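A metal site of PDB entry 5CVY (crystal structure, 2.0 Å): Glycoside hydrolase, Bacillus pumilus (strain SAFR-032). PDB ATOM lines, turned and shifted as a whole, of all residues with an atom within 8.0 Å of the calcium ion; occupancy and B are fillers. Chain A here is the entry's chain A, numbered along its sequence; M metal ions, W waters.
NH2 of Arg 597 lies within salt-bridge range of OD1 of Asp 405 (2.8 Å). The side-chain hydroxyl (OG) of Ser 183 sits close to the side-chain carboxylate (OE2) of Glu 186. OE2 of Glu 186 sits close to NH1 of Arg 597.
Three residues have an atom within 4 Å of the calcium ion: Gln 181, Glu 186 and Asp 405. The nearest printed residue that does not touch the calcium ion is Arg 597 (4.1 Å).
The calcium ion is bound by water W2 (2.3 Å), the side-chain carboxylate (OD2) of Asp 405 (2.3 Å), the backbone carbonyl oxygen (O) of Gln 181 (2.4 Å), the side-chain amide oxygen (OE1) of Gln 181 (2.4 Å), the side-chain carboxylate (OE2) of Glu 186 (2.5 Å), the side-chain carboxylate (OE1) of Glu 186 (2.7 Å) and water W1 (2.9 Å). The calcium ion has seven donor atoms within binding distance.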
ATOM      1  N   PRO A 112       5.349  -3.401  10.465  1.00  0.00           N
ATOM      2  CA  PRO A 112       4.261  -4.369  10.342  1.00  0.00           C
ATOM      3  C   PRO A 112       4.659  -5.808  10.172  1.00  0.00           C
ATOM      4  O   PRO A 112       3.768  -6.663  10.323  1.00  0.00           O
ATOM      5  CB  PRO A 112       3.487  -3.893   9.116  1.00  0.00           C
ATOM      6  CG  PRO A 112       4.496  -3.158   8.319  1.00  0.00           C
ATOM      7  CD  PRO A 112       5.450  -2.535   9.260  1.00  0.00           C
ATOM      8  N   TYR A 113       5.941  -6.080   9.887  1.00  0.00           N
ATOM      9  CA  TYR A 113       6.486  -7.463   9.864  1.00  0.00           C
ATOM     10  C   TYR A 113       7.869  -7.539  10.485  1.00  0.00           C
ATOM     11  O   TYR A 113       8.603  -6.537  10.473  1.00  0.00           O
ATOM     12  CB  TYR A 113       6.642  -7.978   8.399  1.00  0.00           C
ATOM     13  CG  TYR A 113       5.310  -8.049   7.668  1.00  0.00           C
ATOM     14  CD1 TYR A 113       4.435  -9.069   7.926  1.00  0.00           C
ATOM     15  CD2 TYR A 113       4.912  -7.020   6.766  1.00  0.00           C
ATOM     16  CE1 TYR A 113       3.190  -9.109   7.313  1.00  0.00           C
ATOM     17  CE2 TYR A 113       3.693  -7.040   6.127  1.00  0.00           C
ATOM     18  CZ  TYR A 113       2.854  -8.094   6.405  1.00  0.00           C
ATOM     19  OH  TYR A 113       1.653  -8.159   5.794  1.00  0.00           O
ATOM     20  N   PRO A 114       8.204  -8.682  11.106  1.00  0.00           N
ATOM     21  CA  PRO A 114       9.518  -8.808  11.692  1.00  0.00           C
ATOM     22  C   PRO A 114      10.671  -8.605  10.674  1.00  0.00           C
ATOM     23  O   PRO A 114      11.764  -8.138  11.052  1.00  0.00           O
ATOM     24  CB  PRO A 114       9.504 -10.223  12.306  1.00  0.00           C
ATOM     25  CG  PRO A 114       8.092 -10.696  12.295  1.00  0.00           C
ATOM     26  CD  PRO A 114       7.353  -9.857  11.356  1.00  0.00           C
ATOM     27  N   ASP A 115      10.382  -8.912   9.407  1.00  0.00           N
ATOM     28  CA  ASP A 115      11.309  -8.775   8.276  1.00  0.00           C
ATOM     29  C   ASP A 115      11.862  -7.371   8.107  1.00  0.00           C
ATOM     30  O   ASP A 115      12.936  -7.186   7.546  1.00  0.00           O
ATOM     31  CB  ASP A 115      10.585  -9.100   6.985  1.00  0.00           C
ATOM     32  CG  ASP A 115       9.798 -10.445   7.020  1.00  0.00           C
ATOM     33  OD1 ASP A 115       8.941 -10.681   7.949  1.00  0.00           O
ATOM     34  OD2 ASP A 115      10.037 -11.254   6.101  1.00  0.00           O
ATOM     35  N   GLY A 179       7.315  -6.266  16.653  1.00  0.00           N
ATOM     36  CA  GLY A 179       6.087  -5.762  16.162  1.00  0.00           C
ATOM     37  C   GLY A 179       4.964  -6.736  16.177  1.00  0.00           C
ATOM     38  O   GLY A 179       5.076  -7.889  16.732  1.00  0.00           O
ATOM     39  N   GLN A 180       3.899  -6.378  15.474  1.00  0.00           N
ATOM     40  CA  GLN A 180       2.622  -7.004  15.651  1.00  0.00           C
ATOM     41  C   GLN A 180       2.428  -8.321  14.896  1.00  0.00           C
ATOM     42  O   GLN A 180       1.403  -9.012  15.114  1.00  0.00           O
ATOM     43  CB  GLN A 180       1.488  -6.015  15.222  1.00  0.00           C
ATOM     44  CG  GLN A 180       1.314  -5.904  13.700  1.00  0.00           C
ATOM     45  CD  GLN A 180       0.569  -4.657  13.273  1.00  0.00           C
ATOM     46  OE1 GLN A 180       0.242  -3.762  14.105  1.00  0.00           O
ATOM     47  NE2 GLN A 180       0.323  -4.555  11.952  1.00  0.00           N
ATOM     48  N   GLN A 181       3.327  -8.630  13.974  1.00  0.00           N
ATOM     49  CA  GLN A 181       3.307  -9.897  13.284  1.00  0.00           C
ATOM     50  C   GLN A 181       4.344 -10.836  13.841  1.00  0.00           C
ATOM     51  O   GLN A 181       4.530 -11.902  13.308  1.00  0.00           O
ATOM     52  CB  GLN A 181       3.488  -9.734  11.769  1.00  0.00           C
ATOM     53  CG  GLN A 181       2.140  -9.606  11.040  1.00  0.00           C
ATOM     54  CD  GLN A 181       1.326 -10.885  11.129  1.00  0.00           C
ATOM     55  OE1 GLN A 181       1.846 -11.959  11.360  1.00  0.00           O
ATOM     56  NE2 GLN A 181       0.035 -10.772  10.957  1.00  0.00           N
ATOM     57  N   GLU A 182       5.041 -10.490  14.905  1.00  0.00           N
ATOM     58  CA  GLU A 182       5.945 -11.483  15.505  1.00  0.00           C
ATOM     59  C   GLU A 182       5.190 -12.354  16.497  1.00  0.00           C
ATOM     60  O   GLU A 182       5.154 -12.059  17.704  1.00  0.00           O
ATOM     61  CB  GLU A 182       7.127 -10.778  16.189  1.00  0.00           C
ATOM     62  CG  GLU A 182       8.220 -11.704  16.676  1.00  0.00           C
ATOM     63  CD  GLU A 182       9.335 -10.968  17.367  1.00  0.00           C
ATOM     64  OE1 GLU A 182       9.014 -10.154  18.264  1.00  0.00           O
ATOM     65  OE2 GLU A 182      10.508 -11.224  17.053  1.00  0.00           O
ATOM     66  N   SER A 183       4.636 -13.449  16.034  1.00  0.00           N
ATOM     67  CA  SER A 183       4.050 -14.404  16.951  1.00  0.00           C
ATOM     68  C   SER A 183       5.134 -15.034  17.842  1.00  0.00           C
ATOM     69  O   SER A 183       6.328 -14.840  17.652  1.00  0.00           O
ATOM     70  CB  SER A 183       3.348 -15.508  16.191  1.00  0.00           C
ATOM     71  OG  SER A 183       4.210 -16.425  15.608  1.00  0.00           O
ATOM     72  N   VAL A 184       4.684 -15.773  18.815  1.00  0.00           N
ATOM     73  CA  VAL A 184       5.532 -16.539  19.700  1.00  0.00           C
ATOM     74  C   VAL A 184       6.466 -17.465  18.928  1.00  0.00           C
ATOM     75  O   VAL A 184       7.583 -17.718  19.356  1.00  0.00           O
ATOM     76  CB  VAL A 184       4.699 -17.337  20.732  1.00  0.00           C
ATOM     77  CG1 VAL A 184       3.841 -18.392  20.067  1.00  0.00           C
ATOM     78  CG2 VAL A 184       5.611 -17.987  21.801  1.00  0.00           C
ATOM     79  N   TRP A 185       6.011 -17.956  17.802  1.00  0.00           N
ATOM     80  CA  TRP A 185       6.804 -18.853  16.971  1.00  0.00           C
ATOM     81  C   TRP A 185       7.935 -18.158  16.242  1.00  0.00           C
ATOM     82  O   TRP A 185       8.860 -18.792  15.770  1.00  0.00           O
ATOM     83  CB  TRP A 185       5.876 -19.516  15.935  1.00  0.00           C
ATOM     84  CG  TRP A 185       4.744 -20.187  16.564  1.00  0.00           C
ATOM     85  CD1 TRP A 185       3.480 -19.701  16.685  1.00  0.00           C
ATOM     86  CD2 TRP A 185       4.770 -21.439  17.213  1.00  0.00           C
ATOM     87  NE1 TRP A 185       2.696 -20.589  17.331  1.00  0.00           N
ATOM     88  CE2 TRP A 185       3.454 -21.667  17.683  1.00  0.00           C
ATOM     89  CE3 TRP A 185       5.738 -22.388  17.422  1.00  0.00           C
ATOM     90  CZ2 TRP A 185       3.097 -22.814  18.355  1.00  0.00           C
ATOM     91  CZ3 TRP A 185       5.400 -23.556  18.119  1.00  0.00           C
ATOM     92  CH2 TRP A 185       4.084 -23.759  18.585  1.00  0.00           C
ATOM     93  N   GLU A 186       7.895 -16.849  16.154  1.00  0.00           N
ATOM     94  CA  GLU A 186       8.732 -16.050  15.206  1.00  0.00           C
ATOM     95  C   GLU A 186       9.766 -15.189  15.952  1.00  0.00           C
ATOM     96  O   GLU A 186      10.504 -14.456  15.314  1.00  0.00           O
ATOM     97  CB  GLU A 186       7.844 -15.179  14.302  1.00  0.00           C
ATOM     98  CG  GLU A 186       6.972 -15.978  13.352  1.00  0.00           C
ATOM     99  CD  GLU A 186       5.872 -15.105  12.841  1.00  0.00           C
ATOM    100  OE1 GLU A 186       6.067 -14.430  11.792  1.00  0.00           O
ATOM    101  OE2 GLU A 186       4.795 -15.087  13.460  1.00  0.00           O
ATOM    102  N   HIS A 404      -1.236  -9.393  16.173  1.00  0.00           N
ATOM    103  CA  HIS A 404      -2.133  -9.818  15.159  1.00  0.00           C
ATOM    104  C   HIS A 404      -1.975 -11.276  14.835  1.00  0.00           C
ATOM    105  O   HIS A 404      -2.746 -11.775  14.055  1.00  0.00           O
ATOM    106  CB  HIS A 404      -1.880  -9.021  13.885  1.00  0.00           C
ATOM    107  CG  HIS A 404      -2.317  -7.605  13.988  1.00  0.00           C
ATOM    108  ND1 HIS A 404      -2.250  -6.740  12.930  1.00  0.00           N
ATOM    109  CD2 HIS A 404      -2.862  -6.905  15.018  1.00  0.00           C
ATOM    110  CE1 HIS A 404      -2.742  -5.572  13.293  1.00  0.00           C
ATOM    111  NE2 HIS A 404      -3.094  -5.640  14.564  1.00  0.00           N
ATOM    112  N   ASP A 405      -1.008 -11.972  15.430  1.00  0.00           N
ATOM    113  CA  ASP A 405      -0.802 -13.349  15.050  1.00  0.00           C
ATOM    114  C   ASP A 405      -0.697 -14.163  16.329  1.00  0.00           C
ATOM    115  O   ASP A 405       0.378 -14.311  16.895  1.00  0.00           O
ATOM    116  CB  ASP A 405       0.433 -13.414  14.142  1.00  0.00           C
ATOM    117  CG  ASP A 405       0.754 -14.786  13.611  1.00  0.00           C
ATOM    118  OD1 ASP A 405       0.037 -15.757  13.900  1.00  0.00           O
ATOM    119  OD2 ASP A 405       1.758 -14.861  12.865  1.00  0.00           O
ATOM    120  N   PRO A 406      -1.815 -14.689  16.828  1.00  0.00           N
ATOM    121  CA  PRO A 406      -3.156 -14.395  16.385  1.00  0.00           C
ATOM    122  C   PRO A 406      -3.659 -13.041  16.950  1.00  0.00           C
ATOM    123  O   PRO A 406      -3.042 -12.452  17.848  1.00  0.00           O
ATOM    124  CB  PRO A 406      -3.928 -15.540  16.982  1.00  0.00           C
ATOM    125  CG  PRO A 406      -3.214 -15.793  18.304  1.00  0.00           C
ATOM    126  CD  PRO A 406      -1.803 -15.402  18.117  1.00  0.00           C
ATOM    127  N   ARG A 597       3.776 -25.016  13.553  1.00  0.00           N
ATOM    128  CA  ARG A 597       4.667 -23.867  13.615  1.00  0.00           C
ATOM    129  C   ARG A 597       5.999 -24.125  14.358  1.00  0.00           C
ATOM    130  O   ARG A 597       6.876 -23.304  14.302  1.00  0.00           O
ATOM    131  CB  ARG A 597       3.936 -22.632  14.127  1.00  0.00           C
ATOM    132  CG  ARG A 597       2.772 -22.247  13.221  1.00  0.00           C
ATOM    133  CD  ARG A 597       2.061 -21.027  13.670  1.00  0.00           C
ATOM    134  NE  ARG A 597       2.773 -19.837  13.226  1.00  0.00           N
ATOM    135  CZ  ARG A 597       2.302 -18.583  13.317  1.00  0.00           C
ATOM    136  NH1 ARG A 597       3.012 -17.555  12.871  1.00  0.00           N
ATOM    137  NH2 ARG A 597       1.142 -18.365  13.942  1.00  0.00           N
ATOM    138  N   GLU A 602       9.830 -19.719   9.402  1.00  0.00           N
ATOM    139  CA  GLU A 602       9.290 -18.397   9.536  1.00  0.00           C
ATOM    140  C   GLU A 602       9.940 -17.537  10.602  1.00  0.00           C
ATOM    141  O   GLU A 602       9.379 -16.518  10.982  1.00  0.00           O
ATOM    142  CB  GLU A 602       7.804 -18.489   9.783  1.00  0.00           C
ATOM    143  CG  GLU A 602       7.083 -17.290   9.206  1.00  0.00           C
ATOM    144  CD  GLU A 602       5.573 -17.384   9.312  1.00  0.00           C
ATOM    145  OE1 GLU A 602       4.908 -16.580   8.620  1.00  0.00           O
ATOM    146  OE2 GLU A 602       5.055 -18.223  10.102  1.00  0.00           O
ATOM    147  N   ARG A 631       6.898  -8.921   2.558  1.00  0.00           N
ATOM    148  CA  ARG A 631       6.983  -8.439   3.924  1.00  0.00           C
ATOM    149  C   ARG A 631       8.031  -7.368   4.126  1.00  0.00           C
ATOM    150  O   ARG A 631       8.213  -6.893   5.252  1.00  0.00           O
ATOM    151  CB  ARG A 631       7.196  -9.605   4.841  1.00  0.00           C
ATOM    152  CG  ARG A 631       5.992 -10.513   4.805  1.00  0.00           C
ATOM    153  CD  ARG A 631       6.037 -11.593   5.842  1.00  0.00           C
ATOM    154  NE  ARG A 631       5.001 -12.556   5.593  1.00  0.00           N
ATOM    155  CZ  ARG A 631       4.956 -13.808   6.066  1.00  0.00           C
ATOM    156  NH1 ARG A 631       5.908 -14.346   6.880  1.00  0.00           N
ATOM    157  NH2 ARG A 631       3.928 -14.571   5.723  1.00  0.00           N
HETATM  158 CA    CA M   1       3.502 -13.611  11.956  1.00  0.00          CA
HETATM  159  O   HOH W   1       4.940 -12.459   9.717  1.00  0.00           O
HETATM  160  O   HOH W   2       3.176 -14.735   9.994  1.00  0.00           O
